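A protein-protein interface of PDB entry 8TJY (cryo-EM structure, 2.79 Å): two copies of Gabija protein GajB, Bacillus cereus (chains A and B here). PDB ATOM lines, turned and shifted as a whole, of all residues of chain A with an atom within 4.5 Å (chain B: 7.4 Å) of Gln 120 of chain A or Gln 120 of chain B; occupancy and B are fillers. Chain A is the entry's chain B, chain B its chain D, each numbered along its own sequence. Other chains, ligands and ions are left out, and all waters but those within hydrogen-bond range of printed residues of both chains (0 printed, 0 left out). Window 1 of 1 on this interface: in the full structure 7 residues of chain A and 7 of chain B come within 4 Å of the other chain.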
ATOM      1  N   ASN A 105     -15.853  -5.547 -20.399  1.00  0.00           N
ATOM      2  CA  ASN A 105     -15.270  -6.240 -19.257  1.00  0.00           C
ATOM      3  C   ASN A 105     -14.863  -5.257 -18.163  1.00  0.00           C
ATOM      4  O   ASN A 105     -13.853  -5.453 -17.486  1.00  0.00           O
ATOM      5  CB  ASN A 105     -14.071  -7.082 -19.691  1.00  0.00           C
ATOM      6  CG  ASN A 105     -14.475  -8.307 -20.487  1.00  0.00           C
ATOM      7  OD1 ASN A 105     -14.001  -8.519 -21.603  1.00  0.00           O
ATOM      8  ND2 ASN A 105     -15.351  -9.124 -19.916  1.00  0.00           N
ATOM      9  N   GLN A 115      -6.426  -8.371 -12.361  1.00  0.00           N
ATOM     10  CA  GLN A 115      -6.806  -9.760 -12.595  1.00  0.00           C
ATOM     11  C   GLN A 115      -7.290  -9.964 -14.024  1.00  0.00           C
ATOM     12  O   GLN A 115      -6.975 -10.977 -14.654  1.00  0.00           O
ATOM     13  CB  GLN A 115      -7.883 -10.181 -11.597  1.00  0.00           C
ATOM     14  CG  GLN A 115      -7.391 -10.261 -10.162  1.00  0.00           C
ATOM     15  CD  GLN A 115      -8.517 -10.472  -9.170  1.00  0.00           C
ATOM     16  OE1 GLN A 115      -9.619 -10.878  -9.542  1.00  0.00           O
ATOM     17  NE2 GLN A 115      -8.249 -10.194  -7.900  1.00  0.00           N
ATOM     18  N   VAL A 116      -8.070  -9.020 -14.549  1.00  0.00           N
ATOM     19  CA  VAL A 116      -8.504  -9.108 -15.940  1.00  0.00           C
ATOM     20  C   VAL A 116      -7.298  -9.045 -16.867  1.00  0.00           C
ATOM     21  O   VAL A 116      -7.115  -9.902 -17.737  1.00  0.00           O
ATOM     22  CB  VAL A 116      -9.524  -7.997 -16.257  1.00  0.00           C
ATOM     23  CG1 VAL A 116      -9.810  -7.939 -17.751  1.00  0.00           C
ATOM     24  CG2 VAL A 116     -10.810  -8.221 -15.482  1.00  0.00           C
ATOM     25  N   LYS A 118      -4.313  -9.857 -16.374  1.00  0.00           N
ATOM     26  CA  LYS A 118      -3.450 -11.030 -16.272  1.00  0.00           C
ATOM     27  C   LYS A 118      -4.143 -12.291 -16.783  1.00  0.00           C
ATOM     28  O   LYS A 118      -3.714 -12.890 -17.775  1.00  0.00           O
ATOM     29  CB  LYS A 118      -3.003 -11.217 -14.820  1.00  0.00           C
ATOM     30  CG  LYS A 118      -2.027 -12.365 -14.616  1.00  0.00           C
ATOM     31  CD  LYS A 118      -1.203 -12.210 -13.340  1.00  0.00           C
ATOM     32  CE  LYS A 118      -2.011 -11.618 -12.192  1.00  0.00           C
ATOM     33  NZ  LYS A 118      -1.283 -11.704 -10.897  1.00  0.00           N
ATOM     34  N   TYR A 119      -5.218 -12.708 -16.112  1.00  0.00           N
ATOM     35  CA  TYR A 119      -5.889 -13.950 -16.479  1.00  0.00           C
ATOM     36  C   TYR A 119      -6.590 -13.820 -17.825  1.00  0.00           C
ATOM     37  O   TYR A 119      -6.416 -14.664 -18.713  1.00  0.00           O
ATOM     38  CB  TYR A 119      -6.897 -14.332 -15.394  1.00  0.00           C
ATOM     39  CG  TYR A 119      -6.330 -14.313 -13.994  1.00  0.00           C
ATOM     40  CD1 TYR A 119      -5.193 -15.043 -13.672  1.00  0.00           C
ATOM     41  CD2 TYR A 119      -6.928 -13.558 -12.995  1.00  0.00           C
ATOM     42  CE1 TYR A 119      -4.673 -15.024 -12.393  1.00  0.00           C
ATOM     43  CE2 TYR A 119      -6.416 -13.533 -11.713  1.00  0.00           C
ATOM     44  CZ  TYR A 119      -5.289 -14.267 -11.417  1.00  0.00           C
ATOM     45  OH  TYR A 119      -4.775 -14.244 -10.140  1.00  0.00           O
ATOM     46  N   GLN A 120      -7.390 -12.765 -17.994  1.00  0.00           N
ATOM     47  CA  GLN A 120      -8.168 -12.613 -19.216  1.00  0.00           C
ATOM     48  C   GLN A 120      -7.301 -12.151 -20.380  1.00  0.00           C
ATOM     49  O   GLN A 120      -7.601 -12.470 -21.532  1.00  0.00           O
ATOM     50  CB  GLN A 120      -9.315 -11.632 -18.976  1.00  0.00           C
ATOM     51  CG  GLN A 120     -10.246 -12.048 -17.844  1.00  0.00           C
ATOM     52  CD  GLN A 120     -11.604 -11.380 -17.921  1.00  0.00           C
ATOM     53  OE1 GLN A 120     -11.922 -10.698 -18.894  1.00  0.00           O
ATOM     54  NE2 GLN A 120     -12.415 -11.573 -16.887  1.00  0.00           N
ATOM     55  N   ASN A 121      -6.223 -11.416 -20.101  1.00  0.00           N
ATOM     56  CA  ASN A 121      -5.311 -10.924 -21.133  1.00  0.00           C
ATOM     57  C   ASN A 121      -5.993  -9.861 -22.000  1.00  0.00           C
ATOM     58  O   ASN A 121      -5.903  -9.862 -23.229  1.00  0.00           O
ATOM     59  CB  ASN A 121      -4.786 -12.084 -21.988  1.00  0.00           C
ATOM     60  CG  ASN A 121      -3.681 -11.661 -22.934  1.00  0.00           C
ATOM     61  OD1 ASN A 121      -3.133 -12.479 -23.670  1.00  0.00           O
ATOM     62  ND2 ASN A 121      -3.346 -10.377 -22.916  1.00  0.00           N
ATOM     63  N   ILE A 122      -6.682  -8.944 -21.325  1.00  0.00           N
ATOM     64  CA  ILE A 122      -7.325  -7.803 -21.973  1.00  0.00           C
ATOM     65  C   ILE A 122      -7.279  -6.630 -21.007  1.00  0.00           C
ATOM     66  O   ILE A 122      -7.415  -6.803 -19.794  1.00  0.00           O
ATOM     67  CB  ILE A 122      -8.774  -8.131 -22.400  1.00  0.00           C
ATOM     68  CG1 ILE A 122      -9.415  -6.944 -23.125  1.00  0.00           C
ATOM     69  CG2 ILE A 122      -9.613  -8.536 -21.195  1.00  0.00           C
ATOM     70  CD1 ILE A 122      -8.915  -6.754 -24.534  1.00  0.00           C
ATOM     71  N   PRO B  95     -10.749 -11.911 -32.061  1.00  0.00           N
ATOM     72  CA  PRO B  95      -9.340 -11.511 -32.055  1.00  0.00           C
ATOM     73  C   PRO B  95      -8.387 -12.662 -32.334  1.00  0.00           C
ATOM     74  O   PRO B  95      -8.645 -13.822 -32.011  1.00  0.00           O
ATOM     75  CB  PRO B  95      -9.153 -10.988 -30.626  1.00  0.00           C
ATOM     76  CG  PRO B  95     -10.051 -11.861 -29.813  1.00  0.00           C
ATOM     77  CD  PRO B  95     -11.210 -12.265 -30.706  1.00  0.00           C
ATOM     78  N   ASN B  97      -5.312 -12.380 -31.050  1.00  0.00           N
ATOM     79  CA  ASN B  97      -4.345 -12.195 -29.978  1.00  0.00           C
ATOM     80  C   ASN B  97      -4.689 -13.130 -28.828  1.00  0.00           C
ATOM     81  O   ASN B  97      -5.861 -13.274 -28.468  1.00  0.00           O
ATOM     82  CB  ASN B  97      -4.338 -10.745 -29.491  1.00  0.00           C
ATOM     83  CG  ASN B  97      -3.525  -9.831 -30.385  1.00  0.00           C
ATOM     84  OD1 ASN B  97      -4.015  -8.799 -30.841  1.00  0.00           O
ATOM     85  ND2 ASN B  97      -2.276 -10.203 -30.634  1.00  0.00           N
ATOM     86  N   PHE B  98      -3.670 -13.773 -28.268  1.00  0.00           N
ATOM     87  CA  PHE B  98      -3.866 -14.658 -27.130  1.00  0.00           C
ATOM     88  C   PHE B  98      -2.503 -15.122 -26.643  1.00  0.00           C
ATOM     89  O   PHE B  98      -1.528 -15.148 -27.402  1.00  0.00           O
ATOM     90  CB  PHE B  98      -4.753 -15.858 -27.488  1.00  0.00           C
ATOM     91  CG  PHE B  98      -4.351 -16.561 -28.757  1.00  0.00           C
ATOM     92  CD1 PHE B  98      -4.825 -16.132 -29.985  1.00  0.00           C
ATOM     93  CD2 PHE B  98      -3.509 -17.659 -28.718  1.00  0.00           C
ATOM     94  CE1 PHE B  98      -4.461 -16.780 -31.149  1.00  0.00           C
ATOM     95  CE2 PHE B  98      -3.142 -18.309 -29.878  1.00  0.00           C
ATOM     96  CZ  PHE B  98      -3.619 -17.870 -31.095  1.00  0.00           C
ATOM     97  N   THR B  99      -2.447 -15.482 -25.364  1.00  0.00           N
ATOM     98  CA  THR B  99      -1.233 -15.965 -24.721  1.00  0.00           C
ATOM     99  C   THR B  99      -1.478 -17.322 -24.079  1.00  0.00           C
ATOM    100  O   THR B  99      -1.025 -17.596 -22.963  1.00  0.00           O
ATOM    101  CB  THR B  99      -0.729 -14.963 -23.684  1.00  0.00           C
ATOM    102  OG1 THR B  99      -1.831 -14.488 -22.900  1.00  0.00           O
ATOM    103  CG2 THR B  99      -0.048 -13.784 -24.366  1.00  0.00           C
ATOM    104  N   ASP B 104      -7.146 -22.026 -15.619  1.00  0.00           N
ATOM    105  CA  ASP B 104      -7.289 -20.710 -15.006  1.00  0.00           C
ATOM    106  C   ASP B 104      -8.632 -20.079 -15.368  1.00  0.00           C
ATOM    107  O   ASP B 104      -9.357 -19.605 -14.493  1.00  0.00           O
ATOM    108  CB  ASP B 104      -6.136 -19.797 -15.432  1.00  0.00           C
ATOM    109  CG  ASP B 104      -5.981 -19.715 -16.939  1.00  0.00           C
ATOM    110  OD1 ASP B 104      -6.767 -20.370 -17.655  1.00  0.00           O
ATOM    111  OD2 ASP B 104      -5.070 -19.001 -17.407  1.00  0.00           O
ATOM    112  N   ASN B 105      -8.959 -20.078 -16.661  1.00  0.00           N
ATOM    113  CA  ASN B 105     -10.219 -19.543 -17.160  1.00  0.00           C
ATOM    114  C   ASN B 105     -11.034 -20.607 -17.892  1.00  0.00           C
ATOM    115  O   ASN B 105     -11.865 -20.285 -18.743  1.00  0.00           O
ATOM    116  CB  ASN B 105      -9.964 -18.347 -18.076  1.00  0.00           C
ATOM    117  CG  ASN B 105      -9.452 -17.134 -17.325  1.00  0.00           C
ATOM    118  OD1 ASN B 105      -8.397 -16.591 -17.649  1.00  0.00           O
ATOM    119  ND2 ASN B 105     -10.200 -16.700 -16.318  1.00  0.00           N
ATOM    120  N   LYS B 112     -18.868 -20.500 -24.276  1.00  0.00           N
ATOM    121  CA  LYS B 112     -18.067 -19.715 -23.348  1.00  0.00           C
ATOM    122  C   LYS B 112     -16.616 -19.622 -23.795  1.00  0.00           C
ATOM    123  O   LYS B 112     -15.942 -18.641 -23.478  1.00  0.00           O
ATOM    124  CB  LYS B 112     -18.141 -20.310 -21.943  1.00  0.00           C
ATOM    125  CG  LYS B 112     -17.532 -19.421 -20.866  1.00  0.00           C
ATOM    126  CD  LYS B 112     -18.406 -18.211 -20.575  1.00  0.00           C
ATOM    127  CE  LYS B 112     -17.799 -17.336 -19.492  1.00  0.00           C
ATOM    128  NZ  LYS B 112     -17.672 -18.057 -18.196  1.00  0.00           N
ATOM    129  N   LEU B 114     -15.578 -19.264 -26.981  1.00  0.00           N
ATOM    130  CA  LEU B 114     -15.585 -18.128 -27.896  1.00  0.00           C
ATOM    131  C   LEU B 114     -15.767 -16.822 -27.137  1.00  0.00           C
ATOM    132  O   LEU B 114     -15.146 -15.808 -27.471  1.00  0.00           O
ATOM    133  CB  LEU B 114     -16.692 -18.293 -28.938  1.00  0.00           C
ATOM    134  CG  LEU B 114     -16.540 -19.438 -29.943  1.00  0.00           C
ATOM    135  CD1 LEU B 114     -17.256 -20.686 -29.461  1.00  0.00           C
ATOM    136  CD2 LEU B 114     -17.057 -19.024 -31.309  1.00  0.00           C
ATOM    137  N   GLN B 115     -16.625 -16.828 -26.114  1.00  0.00           N
ATOM    138  CA  GLN B 115     -16.841 -15.616 -25.331  1.00  0.00           C
ATOM    139  C   GLN B 115     -15.555 -15.167 -24.649  1.00  0.00           C
ATOM    140  O   GLN B 115     -15.244 -13.972 -24.619  1.00  0.00           O
ATOM    141  CB  GLN B 115     -17.945 -15.846 -24.301  1.00  0.00           C
ATOM    142  CG  GLN B 115     -19.323 -16.044 -24.910  1.00  0.00           C
ATOM    143  CD  GLN B 115     -20.371 -16.400 -23.874  1.00  0.00           C
ATOM    144  OE1 GLN B 115     -20.155 -16.235 -22.674  1.00  0.00           O
ATOM    145  NE2 GLN B 115     -21.516 -16.892 -24.336  1.00  0.00           N
ATOM    146  N   VAL B 116     -14.799 -16.109 -24.086  1.00  0.00           N
ATOM    147  CA  VAL B 116     -13.525 -15.768 -23.458  1.00  0.00           C
ATOM    148  C   VAL B 116     -12.549 -15.250 -24.507  1.00  0.00           C
ATOM    149  O   VAL B 116     -11.938 -14.189 -24.340  1.00  0.00           O
ATOM    150  CB  VAL B 116     -12.957 -16.985 -22.704  1.00  0.00           C
ATOM    151  CG1 VAL B 116     -11.542 -16.710 -22.214  1.00  0.00           C
ATOM    152  CG2 VAL B 116     -13.857 -17.353 -21.536  1.00  0.00           C
ATOM    153  N   LEU B 117     -12.423 -15.967 -25.624  1.00  0.00           N
ATOM    154  CA  LEU B 117     -11.490 -15.549 -26.666  1.00  0.00           C
ATOM    155  C   LEU B 117     -11.811 -14.145 -27.165  1.00  0.00           C
ATOM    156  O   LEU B 117     -10.902 -13.376 -27.499  1.00  0.00           O
ATOM    157  CB  LEU B 117     -11.521 -16.551 -27.821  1.00  0.00           C
ATOM    158  CG  LEU B 117     -10.422 -16.446 -28.882  1.00  0.00           C
ATOM    159  CD1 LEU B 117      -9.033 -16.419 -28.265  1.00  0.00           C
ATOM    160  CD2 LEU B 117     -10.545 -17.597 -29.865  1.00  0.00           C
ATOM    161  N   LYS B 118     -13.095 -13.790 -27.221  1.00  0.00           N
ATOM    162  CA  LYS B 118     -13.490 -12.494 -27.761  1.00  0.00           C
ATOM    163  C   LYS B 118     -13.392 -11.391 -26.712  1.00  0.00           C
ATOM    164  O   LYS B 118     -12.616 -10.441 -26.863  1.00  0.00           O
ATOM    165  CB  LYS B 118     -14.914 -12.582 -28.318  1.00  0.00           C
ATOM    166  CG  LYS B 118     -15.395 -11.313 -29.004  1.00  0.00           C
ATOM    167  CD  LYS B 118     -16.530 -11.581 -29.989  1.00  0.00           C
ATOM    168  CE  LYS B 118     -17.487 -12.661 -29.500  1.00  0.00           C
ATOM    169  NZ  LYS B 118     -18.719 -12.729 -30.331  1.00  0.00           N
ATOM    170  N   TYR B 119     -14.176 -11.501 -25.638  1.00  0.00           N
ATOM    171  CA  TYR B 119     -14.198 -10.454 -24.622  1.00  0.00           C
ATOM    172  C   TYR B 119     -12.908 -10.451 -23.813  1.00  0.00           C
ATOM    173  O   TYR B 119     -12.228  -9.423 -23.711  1.00  0.00           O
ATOM    174  CB  TYR B 119     -15.400 -10.654 -23.700  1.00  0.00           C
ATOM    175  CG  TYR B 119     -16.705 -10.875 -24.429  1.00  0.00           C
ATOM    176  CD1 TYR B 119     -17.152  -9.971 -25.383  1.00  0.00           C
ATOM    177  CD2 TYR B 119     -17.485 -11.992 -24.168  1.00  0.00           C
ATOM    178  CE1 TYR B 119     -18.344 -10.172 -26.052  1.00  0.00           C
ATOM    179  CE2 TYR B 119     -18.677 -12.201 -24.832  1.00  0.00           C
ATOM    180  CZ  TYR B 119     -19.103 -11.290 -25.772  1.00  0.00           C
ATOM    181  OH  TYR B 119     -20.291 -11.497 -26.435  1.00  0.00           O
ATOM    182  N   GLN B 120     -12.555 -11.598 -23.229  1.00  0.00           N
ATOM    183  CA  GLN B 120     -11.376 -11.666 -22.377  1.00  0.00           C
ATOM    184  C   GLN B 120     -10.092 -11.572 -23.189  1.00  0.00           C
ATOM    185  O   GLN B 120      -9.082 -11.075 -22.684  1.00  0.00           O
ATOM    186  CB  GLN B 120     -11.407 -12.960 -21.565  1.00  0.00           C
ATOM    187  CG  GLN B 120     -12.662 -13.120 -20.718  1.00  0.00           C
ATOM    188  CD  GLN B 120     -12.484 -14.100 -19.575  1.00  0.00           C
ATOM    189  OE1 GLN B 120     -11.378 -14.573 -19.312  1.00  0.00           O
ATOM    190  NE2 GLN B 120     -13.576 -14.414 -18.890  1.00  0.00           N
ATOM    191  N   ASN B 121     -10.110 -12.026 -24.443  1.00  0.00           N
ATOM    192  CA  ASN B 121      -8.940 -11.977 -25.321  1.00  0.00           C
ATOM    193  C   ASN B 121      -7.854 -12.938 -24.836  1.00  0.00           C
ATOM    194  O   ASN B 121      -6.670 -12.599 -24.772  1.00  0.00           O
ATOM    195  CB  ASN B 121      -8.402 -10.546 -25.432  1.00  0.00           C
ATOM    196  CG  ASN B 121      -7.323 -10.405 -26.486  1.00  0.00           C
ATOM    197  OD1 ASN B 121      -6.806  -9.314 -26.720  1.00  0.00           O
ATOM    198  ND2 ASN B 121      -6.976 -11.513 -27.130  1.00  0.00           N
ATOM    199  N   ILE B 122      -8.271 -14.154 -24.493  1.00  0.00           N
ATOM    200  CA  ILE B 122      -7.356 -15.221 -24.098  1.00  0.00           C
ATOM    201  C   ILE B 122      -7.952 -16.540 -24.564  1.00  0.00           C
ATOM    202  O   ILE B 122      -9.173 -16.720 -24.558  1.00  0.00           O
ATOM    203  CB  ILE B 122      -7.100 -15.219 -22.574  1.00  0.00           C
ATOM    204  CG1 ILE B 122      -6.110 -16.318 -22.176  1.00  0.00           C
ATOM    205  CG2 ILE B 122      -8.406 -15.382 -21.807  1.00  0.00           C
ATOM    206  CD1 ILE B 122      -4.681 -16.007 -22.546  1.00  0.00           C
ATOM    207  N   LEU B 123      -7.088 -17.463 -24.975  1.00  0.00           N
ATOM    208  CA  LEU B 123      -7.562 -18.736 -25.496  1.00  0.00           C
ATOM    209  C   LEU B 123      -8.281 -19.521 -24.405  1.00  0.00           C
ATOM    210  O   LEU B 123      -7.825 -19.588 -23.260  1.00  0.00           O
ATOM    211  CB  LEU B 123      -6.392 -19.549 -26.051  1.00  0.00           C
ATOM    212  CG  LEU B 123      -6.752 -20.558 -27.142  1.00  0.00           C
ATOM    213  CD1 LEU B 123      -7.128 -19.844 -28.432  1.00  0.00           C
ATOM    214  CD2 LEU B 123      -5.603 -21.520 -27.379  1.00  0.00           C
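The side-chain amide oxygen (OD1) of Asn 105 of chain A lies close to the backbone carbonyl oxygen (O) of Tyr 119 of chain B, 2.9 Å away.
O of Tyr 119 of chain A lies close to OD1 of Asn 105 of chain B, at 3.0 Å.
The backbone carbonyl oxygen (O) of Gln 120 of chain A lies close to the backbone NH (N) of Ile 122 of chain B, at 3.5 Å.
OD1 of Asn 121 of chain A is in hydrogen-bond range of OG1 of Thr 99 of chain B (2.5 Å).
The backbone NH (N) of Ile 122 of chain A sits close to the backbone carbonyl oxygen (O) of Gln 120 of chain B, 3.5 Å away.
O of Gln 120 of chain A lies close to O of Gln 120 of chain B (2.3 Å).
The backbone carbonyl oxygen (O) of Asn 121 of chain B sits close to the backbone carbonyl oxygen (O) of Gln 120 of chain A.
O of Asn 121 of chain A lies close to O of Gln 120 of chain B.
O of Asn 121 of chain A sits close to O of Asn 121 of chain B, at 3.2 Å.
O of Val 116 of chain A sits at hydrogen-bond distance from N of Asn 121 of chain A (2.9 Å).
The backbone carbonyl oxygen of Asn 97 of chain B lies within hydrogen-bond range of the side-chain amide nitrogen of Asn 121 of chain B (2.5 Å).
O of Val 116 of chain B lies within hydrogen-bond range of N of Asn 121 of chain B, at 2.8 Å.
Asn 105 of chain A touches Gln 120 of chain B.
CG2 of Ile 122 of chain B touches O of Tyr 119 of chain A, 3.7 Å away.
Gln 120 of chain A touches Asn 105 of chain B (N to OD1, 3.97 Å).
Asn 121 of chain A touches Ile 122 of chain B (CB to CB, 3.9 Å).
Ile 122 of chain A touches Tyr 119 of chain B (CG2 to O, 3.7 Å).
Ile 122 of chain A touches Asn 121 of chain B.
Gln 120 of chain A touches just these residues of chain B: Asn 105, Gln 120, Asn 121 and Ile 122.
Of chain A, only Asn 105 (3.8 Å), Gln 120 (2.3 Å), Asn 121 (3.4 Å) and Ile 122 (3.0 Å) come within 4 Å of Gln 120 of chain B.
Printed residues of chain A within 4 Å of Ile 122 of chain B: Tyr 119, Gln 120 and Asn 121.
Of the printed residues of chain A, Thr 99 of chain B touches Asn 121.
Of the printed residues of chain B, Asn 105 of chain A touches Tyr 119 (2.9 Å) and Gln 120 (3.8 Å).
The nearest printed residue of chain A that does not touch Thr 99 of chain B is Lys 118 of chain A (5.7 Å).
Hydrophobic or aromatic side chains of chain A within 4 Å of the printed part of chain B: Tyr 119 and Ile 122.
Hydrophobic or aromatic side chains of chain B within 4 Å of the printed part of chain A: Tyr 119 and Ile 122.
Among the printed residues, no Asp or Glu carboxylate lies within 4 Å of a Lys or Arg side-chain nitrogen of the other chain.
Asn 105 of chain A touches Gln 120 of chain B, and with the chains exchanged Gln 120 of chain A touches Asn 105 of chain B.
Tyr 119 of chain A touches Ile 122 of chain B, and with the chains exchanged Ile 122 of chain A touches Tyr 119 of chain B.
Gln 120 of chain A touches Asn 121 of chain B, and with the chains exchanged Asn 121 of chain A touches Gln 120 of chain B.
Gln 120 of chain A touches Ile 122 of chain B, and with the chains exchanged Ile 122 of chain A touches Gln 120 of chain B.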
